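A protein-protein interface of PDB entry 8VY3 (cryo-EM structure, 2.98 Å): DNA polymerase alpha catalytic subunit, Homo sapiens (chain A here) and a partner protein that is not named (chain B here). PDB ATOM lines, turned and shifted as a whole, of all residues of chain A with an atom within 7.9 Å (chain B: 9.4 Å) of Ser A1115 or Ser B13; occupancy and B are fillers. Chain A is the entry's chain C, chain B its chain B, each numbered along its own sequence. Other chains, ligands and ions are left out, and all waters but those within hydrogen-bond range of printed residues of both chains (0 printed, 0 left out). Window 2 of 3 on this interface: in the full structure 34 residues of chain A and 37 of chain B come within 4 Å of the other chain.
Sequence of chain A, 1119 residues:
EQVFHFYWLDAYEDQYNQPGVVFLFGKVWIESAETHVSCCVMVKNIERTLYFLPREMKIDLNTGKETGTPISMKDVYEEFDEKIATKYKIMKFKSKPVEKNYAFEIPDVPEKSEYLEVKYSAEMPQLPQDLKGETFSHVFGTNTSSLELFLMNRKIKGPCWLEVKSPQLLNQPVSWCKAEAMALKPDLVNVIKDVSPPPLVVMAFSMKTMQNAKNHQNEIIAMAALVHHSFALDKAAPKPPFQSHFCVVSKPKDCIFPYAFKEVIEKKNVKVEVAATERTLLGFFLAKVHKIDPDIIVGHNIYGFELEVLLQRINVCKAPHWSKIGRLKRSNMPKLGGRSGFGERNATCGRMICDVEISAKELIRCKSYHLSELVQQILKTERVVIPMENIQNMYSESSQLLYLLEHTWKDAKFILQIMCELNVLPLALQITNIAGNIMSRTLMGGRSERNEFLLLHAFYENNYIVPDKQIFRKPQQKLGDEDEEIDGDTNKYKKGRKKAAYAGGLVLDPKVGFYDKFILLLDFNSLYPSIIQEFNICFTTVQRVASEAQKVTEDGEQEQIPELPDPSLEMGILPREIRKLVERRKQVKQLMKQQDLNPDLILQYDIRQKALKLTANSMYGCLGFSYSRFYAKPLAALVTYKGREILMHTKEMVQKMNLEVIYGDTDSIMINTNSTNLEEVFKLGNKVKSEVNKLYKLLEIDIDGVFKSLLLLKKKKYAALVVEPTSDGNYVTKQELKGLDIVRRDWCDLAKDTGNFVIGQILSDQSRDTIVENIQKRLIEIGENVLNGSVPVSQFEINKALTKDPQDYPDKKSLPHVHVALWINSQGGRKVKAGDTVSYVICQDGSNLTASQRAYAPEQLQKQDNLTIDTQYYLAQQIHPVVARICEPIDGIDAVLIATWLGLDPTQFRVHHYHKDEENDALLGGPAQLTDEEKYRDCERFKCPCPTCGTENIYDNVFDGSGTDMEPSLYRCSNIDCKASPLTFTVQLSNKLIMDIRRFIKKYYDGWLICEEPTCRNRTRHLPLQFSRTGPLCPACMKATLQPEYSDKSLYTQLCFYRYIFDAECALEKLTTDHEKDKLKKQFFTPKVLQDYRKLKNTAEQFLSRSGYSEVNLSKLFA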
ATOM      1  N   VAL A1112      36.683   7.690 -31.663  1.00  0.00           N
ATOM      2  CA  VAL A1112      35.282   7.987 -31.941  1.00  0.00           C
ATOM      3  C   VAL A1112      34.616   8.426 -30.646  1.00  0.00           C
ATOM      4  O   VAL A1112      34.639   7.701 -29.647  1.00  0.00           O
ATOM      5  CB  VAL A1112      34.552   6.781 -32.558  1.00  0.00           C
ATOM      6  CG1 VAL A1112      33.066   7.059 -32.641  1.00  0.00           C
ATOM      7  CG2 VAL A1112      35.105   6.473 -33.928  1.00  0.00           C
ATOM      8  N   ASN A1113      34.023   9.616 -30.654  1.00  0.00           N
ATOM      9  CA  ASN A1113      33.361  10.151 -29.471  1.00  0.00           C
ATOM     10  C   ASN A1113      31.898   9.731 -29.430  1.00  0.00           C
ATOM     11  O   ASN A1113      31.080  10.240 -30.202  1.00  0.00           O
ATOM     12  CB  ASN A1113      33.479  11.674 -29.444  1.00  0.00           C
ATOM     13  CG  ASN A1113      33.269  12.248 -28.063  1.00  0.00           C
ATOM     14  OD1 ASN A1113      33.884  11.804 -27.094  1.00  0.00           O
ATOM     15  ND2 ASN A1113      32.401  13.244 -27.964  1.00  0.00           N
ATOM     16  N   LEU A1114      31.559   8.801 -28.534  1.00  0.00           N
ATOM     17  CA  LEU A1114      30.189   8.307 -28.466  1.00  0.00           C
ATOM     18  C   LEU A1114      29.251   9.312 -27.811  1.00  0.00           C
ATOM     19  O   LEU A1114      28.042   9.281 -28.065  1.00  0.00           O
ATOM     20  CB  LEU A1114      30.146   6.977 -27.717  1.00  0.00           C
ATOM     21  CG  LEU A1114      30.960   5.831 -28.309  1.00  0.00           C
ATOM     22  CD1 LEU A1114      31.118   4.714 -27.299  1.00  0.00           C
ATOM     23  CD2 LEU A1114      30.307   5.318 -29.571  1.00  0.00           C
ATOM     24  N   SER A1115      29.777  10.195 -26.961  1.00  0.00           N
ATOM     25  CA  SER A1115      28.937  11.195 -26.309  1.00  0.00           C
ATOM     26  C   SER A1115      28.315  12.137 -27.330  1.00  0.00           C
ATOM     27  O   SER A1115      27.136  12.493 -27.232  1.00  0.00           O
ATOM     28  CB  SER A1115      29.756  11.977 -25.285  1.00  0.00           C
ATOM     29  OG  SER A1115      30.376  11.108 -24.356  1.00  0.00           O
ATOM     30  N   LYS A1116      29.103  12.562 -28.317  1.00  0.00           N
ATOM     31  CA  LYS A1116      28.573  13.413 -29.377  1.00  0.00           C
ATOM     32  C   LYS A1116      27.722  12.614 -30.352  1.00  0.00           C
ATOM     33  O   LYS A1116      26.843  13.167 -31.023  1.00  0.00           O
ATOM     34  CB  LYS A1116      29.721  14.102 -30.111  1.00  0.00           C
ATOM     35  CG  LYS A1116      29.381  15.474 -30.658  1.00  0.00           C
ATOM     36  CD  LYS A1116      30.472  15.981 -31.583  1.00  0.00           C
ATOM     37  CE  LYS A1116      30.199  15.584 -33.024  1.00  0.00           C
ATOM     38  NZ  LYS A1116      31.443  15.568 -33.843  1.00  0.00           N
ATOM     39  N   LEU A1117      27.971  11.307 -30.449  1.00  0.00           N
ATOM     40  CA  LEU A1117      27.309  10.499 -31.467  1.00  0.00           C
ATOM     41  C   LEU A1117      25.866  10.185 -31.096  1.00  0.00           C
ATOM     42  O   LEU A1117      24.991  10.175 -31.969  1.00  0.00           O
ATOM     43  CB  LEU A1117      28.101   9.212 -31.697  1.00  0.00           C
ATOM     44  CG  LEU A1117      27.600   8.264 -32.779  1.00  0.00           C
ATOM     45  CD1 LEU A1117      27.641   8.959 -34.115  1.00  0.00           C
ATOM     46  CD2 LEU A1117      28.452   7.019 -32.813  1.00  0.00           C
ATOM     47  N   PHE A1118      25.593   9.931 -29.818  1.00  0.00           N
ATOM     48  CA  PHE A1118      24.256   9.566 -29.370  1.00  0.00           C
ATOM     49  C   PHE A1118      23.499  10.697 -28.698  1.00  0.00           C
ATOM     50  O   PHE A1118      22.323  10.896 -29.006  1.00  0.00           O
ATOM     51  CB  PHE A1118      24.321   8.374 -28.402  1.00  0.00           C
ATOM     52  CG  PHE A1118      24.904   7.138 -29.013  1.00  0.00           C
ATOM     53  CD1 PHE A1118      24.329   6.568 -30.131  1.00  0.00           C
ATOM     54  CD2 PHE A1118      26.024   6.545 -28.469  1.00  0.00           C
ATOM     55  CE1 PHE A1118      24.867   5.438 -30.698  1.00  0.00           C
ATOM     56  CE2 PHE A1118      26.563   5.410 -29.032  1.00  0.00           C
ATOM     57  CZ  PHE A1118      25.984   4.858 -30.147  1.00  0.00           C
ATOM     58  N   ALA A1119      24.131  11.444 -27.799  1.00  0.00           N
ATOM     59  CA  ALA A1119      23.459  12.549 -27.129  1.00  0.00           C
ATOM     60  C   ALA A1119      23.363  13.760 -28.049  1.00  0.00           C
ATOM     61  O   ALA A1119      22.641  13.737 -29.046  1.00  0.00           O
ATOM     62  CB  ALA A1119      24.188  12.913 -25.845  1.00  0.00           C
ATOM     63  N   LEU B   9      19.086   1.145 -21.981  1.00  0.00           N
ATOM     64  CA  LEU B   9      18.749   2.519 -21.657  1.00  0.00           C
ATOM     65  C   LEU B   9      20.028   3.247 -21.261  1.00  0.00           C
ATOM     66  O   LEU B   9      21.044   2.613 -20.960  1.00  0.00           O
ATOM     67  CB  LEU B   9      17.719   2.547 -20.521  1.00  0.00           C
ATOM     68  CG  LEU B   9      16.698   3.668 -20.350  1.00  0.00           C
ATOM     69  CD1 LEU B   9      15.519   3.125 -19.558  1.00  0.00           C
ATOM     70  CD2 LEU B   9      17.289   4.869 -19.642  1.00  0.00           C
ATOM     71  N   GLN B  10      19.977   4.583 -21.266  1.00  0.00           N
ATOM     72  CA  GLN B  10      21.127   5.393 -20.873  1.00  0.00           C
ATOM     73  C   GLN B  10      22.322   5.128 -21.783  1.00  0.00           C
ATOM     74  O   GLN B  10      23.223   4.365 -21.416  1.00  0.00           O
ATOM     75  CB  GLN B  10      21.498   5.145 -19.409  1.00  0.00           C
ATOM     76  CG  GLN B  10      20.650   5.917 -18.396  1.00  0.00           C
ATOM     77  CD  GLN B  10      20.235   7.304 -18.871  1.00  0.00           C
ATOM     78  OE1 GLN B  10      21.033   8.054 -19.434  1.00  0.00           O
ATOM     79  NE2 GLN B  10      18.971   7.645 -18.649  1.00  0.00           N
ATOM     80  N   PRO B  11      22.325   5.693 -22.991  1.00  0.00           N
ATOM     81  CA  PRO B  11      23.387   5.413 -23.976  1.00  0.00           C
ATOM     82  C   PRO B  11      24.775   5.553 -23.380  1.00  0.00           C
ATOM     83  O   PRO B  11      24.973   6.287 -22.400  1.00  0.00           O
ATOM     84  CB  PRO B  11      23.147   6.481 -25.052  1.00  0.00           C
ATOM     85  CG  PRO B  11      21.716   6.844 -24.905  1.00  0.00           C
ATOM     86  CD  PRO B  11      21.447   6.784 -23.437  1.00  0.00           C
ATOM     87  N   PRO B  12      25.768   4.866 -23.946  1.00  0.00           N
ATOM     88  CA  PRO B  12      27.139   4.999 -23.438  1.00  0.00           C
ATOM     89  C   PRO B  12      27.684   6.399 -23.677  1.00  0.00           C
ATOM     90  O   PRO B  12      27.349   7.053 -24.666  1.00  0.00           O
ATOM     91  CB  PRO B  12      27.912   3.946 -24.240  1.00  0.00           C
ATOM     92  CG  PRO B  12      27.142   3.822 -25.503  1.00  0.00           C
ATOM     93  CD  PRO B  12      25.704   3.946 -25.094  1.00  0.00           C
ATOM     94  N   SER B  13      28.525   6.857 -22.756  1.00  0.00           N
ATOM     95  CA  SER B  13      29.196   8.143 -22.873  1.00  0.00           C
ATOM     96  C   SER B  13      30.697   7.998 -23.053  1.00  0.00           C
ATOM     97  O   SER B  13      31.425   8.986 -22.928  1.00  0.00           O
ATOM     98  CB  SER B  13      28.903   9.005 -21.643  1.00  0.00           C
ATOM     99  OG  SER B  13      29.569   8.498 -20.500  1.00  0.00           O
ATOM    100  N   GLU B  14      31.171   6.793 -23.352  1.00  0.00           N
ATOM    101  CA  GLU B  14      32.592   6.516 -23.491  1.00  0.00           C
ATOM    102  C   GLU B  14      33.133   7.067 -24.800  1.00  0.00           C
ATOM    103  O   GLU B  14      32.424   7.762 -25.533  1.00  0.00           O
ATOM    104  CB  GLU B  14      32.839   5.009 -23.433  1.00  0.00           C
ATOM    105  CG  GLU B  14      34.018   4.579 -22.594  1.00  0.00           C
ATOM    106  CD  GLU B  14      34.006   3.091 -22.319  1.00  0.00           C
ATOM    107  OE1 GLU B  14      33.229   2.648 -21.449  1.00  0.00           O
ATOM    108  OE2 GLU B  14      34.770   2.359 -22.982  1.00  0.00           O
ATOM    109  N   ASN B  15      34.396   6.770 -25.090  1.00  0.00           N
ATOM    110  CA  ASN B  15      34.934   6.947 -26.431  1.00  0.00           C
ATOM    111  C   ASN B  15      35.800   5.745 -26.792  1.00  0.00           C
ATOM    112  O   ASN B  15      36.435   5.143 -25.920  1.00  0.00           O
ATOM    113  CB  ASN B  15      35.638   8.314 -26.544  1.00  0.00           C
ATOM    114  CG  ASN B  15      37.064   8.344 -25.988  1.00  0.00           C
ATOM    115  OD1 ASN B  15      37.762   7.342 -25.884  1.00  0.00           O
ATOM    116  ND2 ASN B  15      37.499   9.546 -25.628  1.00  0.00           N
ATOM    117  N   ILE B  16      35.786   5.351 -28.059  1.00  0.00           N
ATOM    118  CA  ILE B  16      36.410   4.120 -28.511  1.00  0.00           C
ATOM    119  C   ILE B  16      37.192   4.413 -29.785  1.00  0.00           C
ATOM    120  O   ILE B  16      36.987   5.434 -30.444  1.00  0.00           O
ATOM    121  CB  ILE B  16      35.379   2.997 -28.755  1.00  0.00           C
ATOM    122  CG1 ILE B  16      34.116   3.560 -29.408  1.00  0.00           C
ATOM    123  CG2 ILE B  16      35.028   2.304 -27.454  1.00  0.00           C
ATOM    124  CD1 ILE B  16      33.167   2.500 -29.898  1.00  0.00           C
ATOM    125  N   PHE B  21      35.011   0.148 -32.890  1.00  0.00           N
ATOM    126  CA  PHE B  21      33.702   0.551 -33.388  1.00  0.00           C
ATOM    127  C   PHE B  21      33.242  -0.360 -34.517  1.00  0.00           C
ATOM    128  O   PHE B  21      32.076  -0.764 -34.561  1.00  0.00           O
ATOM    129  CB  PHE B  21      33.749   2.007 -33.850  1.00  0.00           C
ATOM    130  CG  PHE B  21      32.404   2.595 -34.181  1.00  0.00           C
ATOM    131  CD1 PHE B  21      31.796   2.341 -35.396  1.00  0.00           C
ATOM    132  CD2 PHE B  21      31.753   3.412 -33.277  1.00  0.00           C
ATOM    133  CE1 PHE B  21      30.567   2.886 -35.698  1.00  0.00           C
ATOM    134  CE2 PHE B  21      30.525   3.956 -33.574  1.00  0.00           C
ATOM    135  CZ  PHE B  21      29.932   3.694 -34.786  1.00  0.00           C
ATOM    136  N   ARG B  76      30.099  -4.675 -21.366  1.00  0.00           N
ATOM    137  CA  ARG B  76      30.447  -3.448 -22.070  1.00  0.00           C
ATOM    138  C   ARG B  76      30.312  -3.622 -23.579  1.00  0.00           C
ATOM    139  O   ARG B  76      29.759  -2.759 -24.276  1.00  0.00           O
ATOM    140  CB  ARG B  76      31.868  -3.046 -21.677  1.00  0.00           C
ATOM    141  CG  ARG B  76      32.365  -1.759 -22.273  1.00  0.00           C
ATOM    142  CD  ARG B  76      33.842  -1.600 -21.983  1.00  0.00           C
ATOM    143  NE  ARG B  76      34.423  -0.475 -22.700  1.00  0.00           N
ATOM    144  CZ  ARG B  76      34.896  -0.547 -23.936  1.00  0.00           C
ATOM    145  NH1 ARG B  76      34.871  -1.679 -24.620  1.00  0.00           N
ATOM    146  NH2 ARG B  76      35.408   0.543 -24.500  1.00  0.00           N
ATOM    147  N   HIS B  79      26.521  -3.720 -24.457  1.00  0.00           N
ATOM    148  CA  HIS B  79      25.894  -2.402 -24.387  1.00  0.00           C
ATOM    149  C   HIS B  79      26.271  -1.543 -25.591  1.00  0.00           C
ATOM    150  O   HIS B  79      25.400  -0.999 -26.295  1.00  0.00           O
ATOM    151  CB  HIS B  79      26.319  -1.722 -23.086  1.00  0.00           C
ATOM    152  CG  HIS B  79      25.555  -0.477 -22.766  1.00  0.00           C
ATOM    153  ND1 HIS B  79      26.006   0.454 -21.857  1.00  0.00           N
ATOM    154  CD2 HIS B  79      24.367  -0.016 -23.218  1.00  0.00           C
ATOM    155  CE1 HIS B  79      25.135   1.441 -21.772  1.00  0.00           C
ATOM    156  NE2 HIS B  79      24.130   1.180 -22.586  1.00  0.00           N
ATOM    157  N   ILE B  80      27.574  -1.421 -25.850  1.00  0.00           N
ATOM    158  CA  ILE B  80      28.046  -0.532 -26.903  1.00  0.00           C
ATOM    159  C   ILE B  80      27.569  -1.047 -28.253  1.00  0.00           C
ATOM    160  O   ILE B  80      27.175  -0.257 -29.114  1.00  0.00           O
ATOM    161  CB  ILE B  80      29.575  -0.380 -26.871  1.00  0.00           C
ATOM    162  CG1 ILE B  80      30.021   0.215 -25.539  1.00  0.00           C
ATOM    163  CG2 ILE B  80      30.035   0.533 -27.984  1.00  0.00           C
ATOM    164  CD1 ILE B  80      31.499   0.117 -25.310  1.00  0.00           C
ATOM    165  N   PHE B  83      23.823  -0.190 -28.854  1.00  0.00           N
ATOM    166  CA  PHE B  83      23.554   1.215 -29.141  1.00  0.00           C
ATOM    167  C   PHE B  83      24.162   1.640 -30.472  1.00  0.00           C
ATOM    168  O   PHE B  83      23.639   2.531 -31.149  1.00  0.00           O
ATOM    169  CB  PHE B  83      24.047   2.089 -27.996  1.00  0.00           C
ATOM    170  CG  PHE B  83      22.993   2.367 -26.979  1.00  0.00           C
ATOM    171  CD1 PHE B  83      22.855   1.556 -25.872  1.00  0.00           C
ATOM    172  CD2 PHE B  83      22.113   3.414 -27.151  1.00  0.00           C
ATOM    173  CE1 PHE B  83      21.879   1.800 -24.942  1.00  0.00           C
ATOM    174  CE2 PHE B  83      21.133   3.661 -26.224  1.00  0.00           C
ATOM    175  CZ  PHE B  83      21.015   2.852 -25.118  1.00  0.00           C
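Asn B15 touches Val A1112 (CA to O, 3.3 Å).
Phe B21 touches Val A1112 (CD2 to CG1, 3.9 Å).
Asn A1113 touches Asn B15 (OD1 to CB, 3.9 Å).
Leu A1114 touches Ile B16.
N of Ser A1115 touches O of Glu B14, at 3.9 Å.
Phe B21 touches Leu A1117.
Phe A1118 touches Pro B12.
CE1 of Phe A1118 touches O of Phe B83, 3.2 Å away.
N of Val A1112 is in hydrogen-bond range of O of Ile B16, 2.6 Å away.
The backbone carbonyl oxygen of Glu B14 sits close to the backbone NH of Leu A1114 (3.3 Å).
O of Ser B13 lies within hydrogen-bond range of OG of Ser A1115, 2.8 Å away.
The side-chain carboxylate of Glu B14 is in salt-bridge range of the guanidinium group of Arg B76, at 2.5 Å.
The side-chain amide nitrogen (ND2) of Asn A1113 sits close to the backbone NH (N) of Lys A1116 (3.4 Å).
Printed residues of chain A that touch a printed residue of chain B: Val A1112, Asn A1113, Leu A1114, Ser A1115, Leu A1117 and Phe A1118.
Hydrophobic or aromatic side chains of chain A that line the printed part of chain B: Val A1112, Leu A1114, Leu A1117 and Phe A1118.
Of the 13 printed residues of chain B, 7 touch a printed residue of chain A.
Among the printed residues, no Asp or Glu carboxylate lies within 4 Å of a Lys or Arg side-chain nitrogen of the other chain.
Ser A1115 touches just these residues of chain B: Ser B13 (2.8 Å) and Glu B14 (3.9 Å).
Of chain A, only Ser A1115 (2.8 Å) comes within 4 Å of Ser B13.
No residue of chain B comes within 4 Å of Ala A1119.
Printed residues of chain A within 4 Å of Phe B83: Phe A1118.
Of the printed residues of chain B, Val A1112 touches Asn B15 (3.3 Å), Ile B16 (2.6 Å) and Phe B21 (3.9 Å).
Of the printed residues of chain B, Leu A1114 touches Glu B14 and Ile B16.
Printed residues of chain A within 4 Å of Phe B21: Val A1112 and Leu A1117.
His B79 touches none of the printed residues of chain A.
Lys A1116 touches none of the printed residues of chain B.
The nearest residue of chain B that does not touch Ser A1115 is Pro B12 (4.6 Å).
The nearest residue of chain A that does not touch Ser B13 is Leu A1114 (4.8 Å).
The nearest printed residue of chain A that does not touch Ile B16 is Asn A1113 (5.1 Å).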
